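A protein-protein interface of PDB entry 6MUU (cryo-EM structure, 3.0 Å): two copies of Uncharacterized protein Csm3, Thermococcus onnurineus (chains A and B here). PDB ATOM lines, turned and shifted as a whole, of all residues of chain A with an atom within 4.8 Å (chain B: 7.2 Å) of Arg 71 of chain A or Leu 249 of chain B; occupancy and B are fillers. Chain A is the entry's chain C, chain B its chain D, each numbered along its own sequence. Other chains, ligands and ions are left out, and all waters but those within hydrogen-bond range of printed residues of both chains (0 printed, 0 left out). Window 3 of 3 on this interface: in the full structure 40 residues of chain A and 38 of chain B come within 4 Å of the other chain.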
ATOM      1  N   LEU A  67     -25.812  26.521  29.560  1.00  0.00           N
ATOM      2  CA  LEU A  67     -24.529  25.778  29.427  1.00  0.00           C
ATOM      3  C   LEU A  67     -24.545  24.563  30.369  1.00  0.00           C
ATOM      4  O   LEU A  67     -24.118  23.478  29.927  1.00  0.00           O
ATOM      5  CB  LEU A  67     -23.379  26.727  29.776  1.00  0.00           C
ATOM      6  CG  LEU A  67     -21.974  26.145  29.620  1.00  0.00           C
ATOM      7  CD1 LEU A  67     -21.737  25.023  30.619  1.00  0.00           C
ATOM      8  CD2 LEU A  67     -21.747  25.653  28.199  1.00  0.00           C
ATOM      9  N   VAL A  68     -25.044  24.721  31.599  1.00  0.00           N
ATOM     10  CA  VAL A  68     -25.081  23.645  32.584  1.00  0.00           C
ATOM     11  C   VAL A  68     -26.237  22.696  32.300  1.00  0.00           C
ATOM     12  O   VAL A  68     -26.129  21.491  32.555  1.00  0.00           O
ATOM     13  CB  VAL A  68     -25.134  24.259  33.997  1.00  0.00           C
ATOM     14  CG1 VAL A  68     -25.313  23.215  35.088  1.00  0.00           C
ATOM     15  CG2 VAL A  68     -23.860  25.002  34.263  1.00  0.00           C
ATOM     16  N   ASN A  69     -27.322  23.199  31.703  1.00  0.00           N
ATOM     17  CA  ASN A  69     -28.446  22.352  31.314  1.00  0.00           C
ATOM     18  C   ASN A  69     -28.044  21.322  30.267  1.00  0.00           C
ATOM     19  O   ASN A  69     -28.611  20.227  30.221  1.00  0.00           O
ATOM     20  CB  ASN A  69     -29.568  23.216  30.759  1.00  0.00           C
ATOM     21  CG  ASN A  69     -30.875  22.489  30.680  1.00  0.00           C
ATOM     22  OD1 ASN A  69     -31.024  21.402  31.213  1.00  0.00           O
ATOM     23  ND2 ASN A  69     -31.823  23.069  29.967  1.00  0.00           N
ATOM     24  N   SER A  70     -27.064  21.643  29.434  1.00  0.00           N
ATOM     25  CA  SER A  70     -26.592  20.730  28.410  1.00  0.00           C
ATOM     26  C   SER A  70     -25.544  19.751  28.909  1.00  0.00           C
ATOM     27  O   SER A  70     -25.186  18.830  28.170  1.00  0.00           O
ATOM     28  CB  SER A  70     -26.013  21.518  27.241  1.00  0.00           C
ATOM     29  OG  SER A  70     -27.010  22.292  26.604  1.00  0.00           O
ATOM     30  N   ARG A  71     -25.039  19.917  30.125  1.00  0.00           N
ATOM     31  CA  ARG A  71     -23.926  19.117  30.617  1.00  0.00           C
ATOM     32  C   ARG A  71     -24.206  18.568  32.004  1.00  0.00           C
ATOM     33  O   ARG A  71     -23.306  18.466  32.840  1.00  0.00           O
ATOM     34  CB  ARG A  71     -22.634  19.929  30.621  1.00  0.00           C
ATOM     35  CG  ARG A  71     -22.082  20.222  29.248  1.00  0.00           C
ATOM     36  CD  ARG A  71     -21.534  18.949  28.655  1.00  0.00           C
ATOM     37  NE  ARG A  71     -20.925  19.133  27.346  1.00  0.00           N
ATOM     38  CZ  ARG A  71     -21.581  18.985  26.203  1.00  0.00           C
ATOM     39  NH1 ARG A  71     -22.865  18.660  26.214  1.00  0.00           N
ATOM     40  NH2 ARG A  71     -20.953  19.158  25.049  1.00  0.00           N
ATOM     41  N   LEU A  72     -25.456  18.188  32.273  1.00  0.00           N
ATOM     42  CA  LEU A  72     -25.788  17.666  33.594  1.00  0.00           C
ATOM     43  C   LEU A  72     -25.246  16.263  33.805  1.00  0.00           C
ATOM     44  O   LEU A  72     -24.925  15.891  34.937  1.00  0.00           O
ATOM     45  CB  LEU A  72     -27.295  17.673  33.810  1.00  0.00           C
ATOM     46  CG  LEU A  72     -27.931  19.049  33.942  1.00  0.00           C
ATOM     47  CD1 LEU A  72     -29.429  18.934  34.017  1.00  0.00           C
ATOM     48  CD2 LEU A  72     -27.400  19.727  35.171  1.00  0.00           C
ATOM     49  N   GLY A  73     -25.140  15.468  32.739  1.00  0.00           N
ATOM     50  CA  GLY A  73     -24.606  14.128  32.886  1.00  0.00           C
ATOM     51  C   GLY A  73     -23.106  14.096  33.059  1.00  0.00           C
ATOM     52  O   GLY A  73     -22.585  13.249  33.790  1.00  0.00           O
ATOM     53  N   GLU A  74     -22.394  15.011  32.409  1.00  0.00           N
ATOM     54  CA  GLU A  74     -20.941  14.984  32.430  1.00  0.00           C
ATOM     55  C   GLU A  74     -20.351  15.686  33.643  1.00  0.00           C
ATOM     56  O   GLU A  74     -19.161  15.506  33.921  1.00  0.00           O
ATOM     57  CB  GLU A  74     -20.386  15.619  31.153  1.00  0.00           C
ATOM     58  CG  GLU A  74     -20.620  14.801  29.891  1.00  0.00           C
ATOM     59  CD  GLU A  74     -21.988  15.027  29.266  1.00  0.00           C
ATOM     60  OE1 GLU A  74     -22.742  15.888  29.762  1.00  0.00           O
ATOM     61  OE2 GLU A  74     -22.314  14.333  28.282  1.00  0.00           O
ATOM     62  N   TRP A  75     -21.142  16.477  34.370  1.00  0.00           N
ATOM     63  CA  TRP A  75     -20.637  17.231  35.509  1.00  0.00           C
ATOM     64  C   TRP A  75     -21.210  16.746  36.836  1.00  0.00           C
ATOM     65  O   TRP A  75     -21.241  17.512  37.802  1.00  0.00           O
ATOM     66  CB  TRP A  75     -20.927  18.724  35.367  1.00  0.00           C
ATOM     67  CG  TRP A  75     -20.222  19.434  34.266  1.00  0.00           C
ATOM     68  CD1 TRP A  75     -19.404  18.896  33.325  1.00  0.00           C
ATOM     69  CD2 TRP A  75     -20.234  20.841  34.032  1.00  0.00           C
ATOM     70  NE1 TRP A  75     -18.935  19.878  32.491  1.00  0.00           N
ATOM     71  CE2 TRP A  75     -19.426  21.084  32.911  1.00  0.00           C
ATOM     72  CE3 TRP A  75     -20.862  21.920  34.655  1.00  0.00           C
ATOM     73  CZ2 TRP A  75     -19.232  22.360  32.400  1.00  0.00           C
ATOM     74  CZ3 TRP A  75     -20.664  23.182  34.147  1.00  0.00           C
ATOM     75  CH2 TRP A  75     -19.854  23.393  33.031  1.00  0.00           C
ATOM     76  N   ARG B   5     -31.571  23.556  25.382  1.00  0.00           N
ATOM     77  CA  ARG B   5     -30.201  23.092  25.526  1.00  0.00           C
ATOM     78  C   ARG B   5     -29.326  23.752  24.476  1.00  0.00           C
ATOM     79  O   ARG B   5     -29.799  24.200  23.434  1.00  0.00           O
ATOM     80  CB  ARG B   5     -30.114  21.568  25.420  1.00  0.00           C
ATOM     81  CG  ARG B   5     -30.659  20.869  26.644  1.00  0.00           C
ATOM     82  CD  ARG B   5     -30.605  19.366  26.531  1.00  0.00           C
ATOM     83  NE  ARG B   5     -31.564  18.900  25.541  1.00  0.00           N
ATOM     84  CZ  ARG B   5     -31.225  18.260  24.432  1.00  0.00           C
ATOM     85  NH1 ARG B   5     -32.158  17.873  23.574  1.00  0.00           N
ATOM     86  NH2 ARG B   5     -29.951  17.993  24.191  1.00  0.00           N
ATOM     87  N   PHE B   6     -28.035  23.805  24.769  1.00  0.00           N
ATOM     88  CA  PHE B   6     -27.064  24.516  23.953  1.00  0.00           C
ATOM     89  C   PHE B   6     -25.989  23.544  23.503  1.00  0.00           C
ATOM     90  O   PHE B   6     -25.393  22.850  24.331  1.00  0.00           O
ATOM     91  CB  PHE B   6     -26.445  25.666  24.747  1.00  0.00           C
ATOM     92  CG  PHE B   6     -25.458  26.476  23.975  1.00  0.00           C
ATOM     93  CD1 PHE B   6     -25.879  27.390  23.030  1.00  0.00           C
ATOM     94  CD2 PHE B   6     -24.103  26.332  24.207  1.00  0.00           C
ATOM     95  CE1 PHE B   6     -24.964  28.133  22.327  1.00  0.00           C
ATOM     96  CE2 PHE B   6     -23.187  27.067  23.506  1.00  0.00           C
ATOM     97  CZ  PHE B   6     -23.616  27.968  22.567  1.00  0.00           C
ATOM     98  N   TYR B   7     -25.742  23.488  22.200  1.00  0.00           N
ATOM     99  CA  TYR B   7     -24.673  22.659  21.668  1.00  0.00           C
ATOM    100  C   TYR B   7     -23.545  23.446  21.036  1.00  0.00           C
ATOM    101  O   TYR B   7     -22.484  22.874  20.780  1.00  0.00           O
ATOM    102  CB  TYR B   7     -25.222  21.667  20.638  1.00  0.00           C
ATOM    103  CG  TYR B   7     -25.963  20.525  21.263  1.00  0.00           C
ATOM    104  CD1 TYR B   7     -25.271  19.470  21.835  1.00  0.00           C
ATOM    105  CD2 TYR B   7     -27.348  20.491  21.282  1.00  0.00           C
ATOM    106  CE1 TYR B   7     -25.935  18.416  22.416  1.00  0.00           C
ATOM    107  CE2 TYR B   7     -28.023  19.440  21.860  1.00  0.00           C
ATOM    108  CZ  TYR B   7     -27.309  18.404  22.426  1.00  0.00           C
ATOM    109  OH  TYR B   7     -27.972  17.348  23.003  1.00  0.00           O
ATOM    110  N   GLY B   8     -23.735  24.730  20.784  1.00  0.00           N
ATOM    111  CA  GLY B   8     -22.726  25.503  20.102  1.00  0.00           C
ATOM    112  C   GLY B   8     -23.337  26.418  19.073  1.00  0.00           C
ATOM    113  O   GLY B   8     -24.558  26.450  18.919  1.00  0.00           O
ATOM    114  N   LYS B   9     -22.506  27.166  18.365  1.00  0.00           N
ATOM    115  CA  LYS B   9     -22.979  28.160  17.420  1.00  0.00           C
ATOM    116  C   LYS B   9     -22.291  27.966  16.084  1.00  0.00           C
ATOM    117  O   LYS B   9     -21.083  27.735  16.031  1.00  0.00           O
ATOM    118  CB  LYS B   9     -22.709  29.573  17.921  1.00  0.00           C
ATOM    119  CG  LYS B   9     -23.453  29.943  19.180  1.00  0.00           C
ATOM    120  CD  LYS B   9     -23.149  31.363  19.560  1.00  0.00           C
ATOM    121  CE  LYS B   9     -23.904  31.818  20.785  1.00  0.00           C
ATOM    122  NZ  LYS B   9     -23.436  31.162  22.022  1.00  0.00           N
ATOM    123  N   PHE B 246     -18.046  26.419  12.998  1.00  0.00           N
ATOM    124  CA  PHE B 246     -18.848  25.869  14.084  1.00  0.00           C
ATOM    125  C   PHE B 246     -18.042  25.939  15.373  1.00  0.00           C
ATOM    126  O   PHE B 246     -17.008  25.280  15.503  1.00  0.00           O
ATOM    127  CB  PHE B 246     -19.265  24.435  13.774  1.00  0.00           C
ATOM    128  CG  PHE B 246     -19.953  23.743  14.911  1.00  0.00           C
ATOM    129  CD1 PHE B 246     -21.210  24.132  15.310  1.00  0.00           C
ATOM    130  CD2 PHE B 246     -19.349  22.686  15.567  1.00  0.00           C
ATOM    131  CE1 PHE B 246     -21.848  23.503  16.358  1.00  0.00           C
ATOM    132  CE2 PHE B 246     -19.991  22.044  16.607  1.00  0.00           C
ATOM    133  CZ  PHE B 246     -21.242  22.456  16.999  1.00  0.00           C
ATOM    134  N   ARG B 247     -18.512  26.745  16.320  1.00  0.00           N
ATOM    135  CA  ARG B 247     -17.894  26.819  17.635  1.00  0.00           C
ATOM    136  C   ARG B 247     -18.577  25.823  18.556  1.00  0.00           C
ATOM    137  O   ARG B 247     -19.766  25.988  18.844  1.00  0.00           O
ATOM    138  CB  ARG B 247     -18.016  28.214  18.222  1.00  0.00           C
ATOM    139  CG  ARG B 247     -17.011  29.230  17.719  1.00  0.00           C
ATOM    140  CD  ARG B 247     -17.448  29.882  16.429  1.00  0.00           C
ATOM    141  NE  ARG B 247     -16.489  30.883  15.986  1.00  0.00           N
ATOM    142  CZ  ARG B 247     -16.501  32.149  16.380  1.00  0.00           C
ATOM    143  NH1 ARG B 247     -17.426  32.575  17.227  1.00  0.00           N
ATOM    144  NH2 ARG B 247     -15.589  32.992  15.924  1.00  0.00           N
ATOM    145  N   PRO B 248     -17.867  24.774  18.958  1.00  0.00           N
ATOM    146  CA  PRO B 248     -18.399  23.737  19.843  1.00  0.00           C
ATOM    147  C   PRO B 248     -18.525  24.290  21.268  1.00  0.00           C
ATOM    148  O   PRO B 248     -17.912  25.291  21.546  1.00  0.00           O
ATOM    149  CB  PRO B 248     -17.373  22.600  19.781  1.00  0.00           C
ATOM    150  CG  PRO B 248     -16.093  23.288  19.397  1.00  0.00           C
ATOM    151  CD  PRO B 248     -16.527  24.419  18.492  1.00  0.00           C
ATOM    152  N   LEU B 249     -19.265  23.613  22.137  1.00  0.00           N
ATOM    153  CA  LEU B 249     -19.458  24.096  23.529  1.00  0.00           C
ATOM    154  C   LEU B 249     -18.095  24.162  24.227  1.00  0.00           C
ATOM    155  O   LEU B 249     -17.849  25.159  24.934  1.00  0.00           O
ATOM    156  CB  LEU B 249     -20.399  23.128  24.255  1.00  0.00           C
ATOM    157  CG  LEU B 249     -20.781  23.525  25.680  1.00  0.00           C
ATOM    158  CD1 LEU B 249     -21.861  22.604  26.229  1.00  0.00           C
ATOM    159  CD2 LEU B 249     -19.563  23.520  26.591  1.00  0.00           C
ATOM    160  N   ASP B 250     -17.235  23.173  24.015  1.00  0.00           N
ATOM    161  CA  ASP B 250     -15.896  23.167  24.655  1.00  0.00           C
ATOM    162  C   ASP B 250     -15.143  24.440  24.252  1.00  0.00           C
ATOM    163  O   ASP B 250     -14.313  24.889  25.050  1.00  0.00           O
ATOM    164  CB  ASP B 250     -15.106  21.900  24.317  1.00  0.00           C
ATOM    165  CG  ASP B 250     -13.999  21.587  25.310  1.00  0.00           C
ATOM    166  OD1 ASP B 250     -14.103  22.042  26.466  1.00  0.00           O
ATOM    167  OD2 ASP B 250     -13.039  20.887  24.921  1.00  0.00           O
ATOM    168  N   TYR B 251     -15.338  24.962  23.048  1.00  0.00           N
ATOM    169  CA  TYR B 251     -14.619  26.168  22.647  1.00  0.00           C
ATOM    170  C   TYR B 251     -14.697  27.247  23.715  1.00  0.00           C
ATOM    171  O   TYR B 251     -13.697  27.905  24.016  1.00  0.00           O
ATOM    172  CB  TYR B 251     -15.179  26.705  21.333  1.00  0.00           C
ATOM    173  CG  TYR B 251     -14.567  28.016  20.902  1.00  0.00           C
ATOM    174  CD1 TYR B 251     -13.292  28.060  20.383  1.00  0.00           C
ATOM    175  CD2 TYR B 251     -15.273  29.208  21.006  1.00  0.00           C
ATOM    176  CE1 TYR B 251     -12.722  29.252  19.987  1.00  0.00           C
ATOM    177  CE2 TYR B 251     -14.712  30.406  20.614  1.00  0.00           C
ATOM    178  CZ  TYR B 251     -13.438  30.419  20.104  1.00  0.00           C
ATOM    179  OH  TYR B 251     -12.878  31.607  19.709  1.00  0.00           O
ATOM    180  N   TYR B 252     -15.875  27.444  24.292  1.00  0.00           N
ATOM    181  CA  TYR B 252     -16.055  28.488  25.281  1.00  0.00           C
ATOM    182  C   TYR B 252     -15.515  28.083  26.640  1.00  0.00           C
ATOM    183  O   TYR B 252     -15.256  28.953  27.475  1.00  0.00           O
ATOM    184  CB  TYR B 252     -17.533  28.841  25.380  1.00  0.00           C
ATOM    185  CG  TYR B 252     -18.089  29.300  24.063  1.00  0.00           C
ATOM    186  CD1 TYR B 252     -17.845  30.577  23.601  1.00  0.00           C
ATOM    187  CD2 TYR B 252     -18.841  28.448  23.270  1.00  0.00           C
ATOM    188  CE1 TYR B 252     -18.343  31.001  22.392  1.00  0.00           C
ATOM    189  CE2 TYR B 252     -19.344  28.864  22.062  1.00  0.00           C
ATOM    190  CZ  TYR B 252     -19.088  30.137  21.628  1.00  0.00           C
ATOM    191  OH  TYR B 252     -19.592  30.541  20.425  1.00  0.00           O
ATOM    192  N   ARG B 253     -15.343  26.785  26.875  1.00  0.00           N
ATOM    193  CA  ARG B 253     -14.716  26.320  28.105  1.00  0.00           C
ATOM    194  C   ARG B 253     -13.226  26.623  28.105  1.00  0.00           C
ATOM    195  O   ARG B 253     -12.728  27.363  28.959  1.00  0.00           O
ATOM    196  CB  ARG B 253     -14.931  24.819  28.271  1.00  0.00           C
ATOM    197  CG  ARG B 253     -16.353  24.372  28.466  1.00  0.00           C
ATOM    198  CD  ARG B 253     -16.885  24.775  29.815  1.00  0.00           C
ATOM    199  NE  ARG B 253     -15.971  24.440  30.908  1.00  0.00           N
ATOM    200  CZ  ARG B 253     -15.790  23.224  31.421  1.00  0.00           C
ATOM    201  NH1 ARG B 253     -14.941  23.062  32.426  1.00  0.00           N
ATOM    202  NH2 ARG B 253     -16.409  22.164  30.921  1.00  0.00           N
ATOM    203  N   THR B 254     -12.497  26.052  27.150  1.00  0.00           N
ATOM    204  CA  THR B 254     -11.044  26.047  27.194  1.00  0.00           C
ATOM    205  C   THR B 254     -10.403  27.169  26.394  1.00  0.00           C
ATOM    206  O   THR B 254      -9.186  27.337  26.479  1.00  0.00           O
ATOM    207  CB  THR B 254     -10.498  24.701  26.697  1.00  0.00           C
ATOM    208  OG1 THR B 254      -9.098  24.623  26.989  1.00  0.00           O
ATOM    209  CG2 THR B 254     -10.686  24.564  25.200  1.00  0.00           C
ATOM    210  N   LYS B 287     -18.542  15.923  15.292  1.00  0.00           N
ATOM    211  CA  LYS B 287     -18.406  16.413  16.659  1.00  0.00           C
ATOM    212  C   LYS B 287     -19.735  16.382  17.399  1.00  0.00           C
ATOM    213  O   LYS B 287     -19.771  16.102  18.602  1.00  0.00           O
ATOM    214  CB  LYS B 287     -17.827  17.827  16.657  1.00  0.00           C
ATOM    215  CG  LYS B 287     -16.390  17.890  16.183  1.00  0.00           C
ATOM    216  CD  LYS B 287     -15.867  19.312  16.183  1.00  0.00           C
ATOM    217  CE  LYS B 287     -15.639  19.812  17.597  1.00  0.00           C
ATOM    218  NZ  LYS B 287     -14.509  19.115  18.264  1.00  0.00           N
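OG of Ser 70 of chain A lies within hydrogen-bond range of N of Phe 6 of chain B (2.6 Å).
Among the printed residues, pairs that only touch across the chains: Leu 67 of chain A with Leu 249 of chain B (3.4 Å), Ser 70 of chain A with Arg 5 of chain B (3.4 Å), Arg 71 of chain A with Leu 249 of chain B (3.6 Å) and Trp 75 of chain A with Arg 253 of chain B (3.2 Å).
Of chain B, only Leu 249 comes within 4 Å of Arg 71 of chain A. Leu 249 of chain B touches just these residues of chain A: Leu 67 (3.4 Å) and Arg 71 (3.6 Å). Printed residues of chain A within 4 Å of Phe 6 of chain B: Ser 70. Of the printed residues of chain A, Arg 5 of chain B touches Ser 70. Of the printed residues of chain B, Ser 70 of chain A touches Arg 5 (3.4 Å) and Phe 6 (2.6 Å).
Printed residues of chain A that touch a printed residue of chain B: Leu 67, Ser 70, Arg 71 and Trp 75. Hydrophobic or aromatic side chains of chain A that line the printed part of chain B: Leu 67 and Trp 75. Of the 15 printed residues of chain B, 4 touch a printed residue of chain A. Hydrophobic or aromatic side chains of chain B within 4 Å of the printed part of chain A: Phe 6 and Leu 249. Among the printed residues, 5 pairs touch across the chains. Among the printed residues, no Asp or Glu carboxylate lies within 4 Å of a Lys or Arg side-chain nitrogen of the other chain.
No position is printed for both chains.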
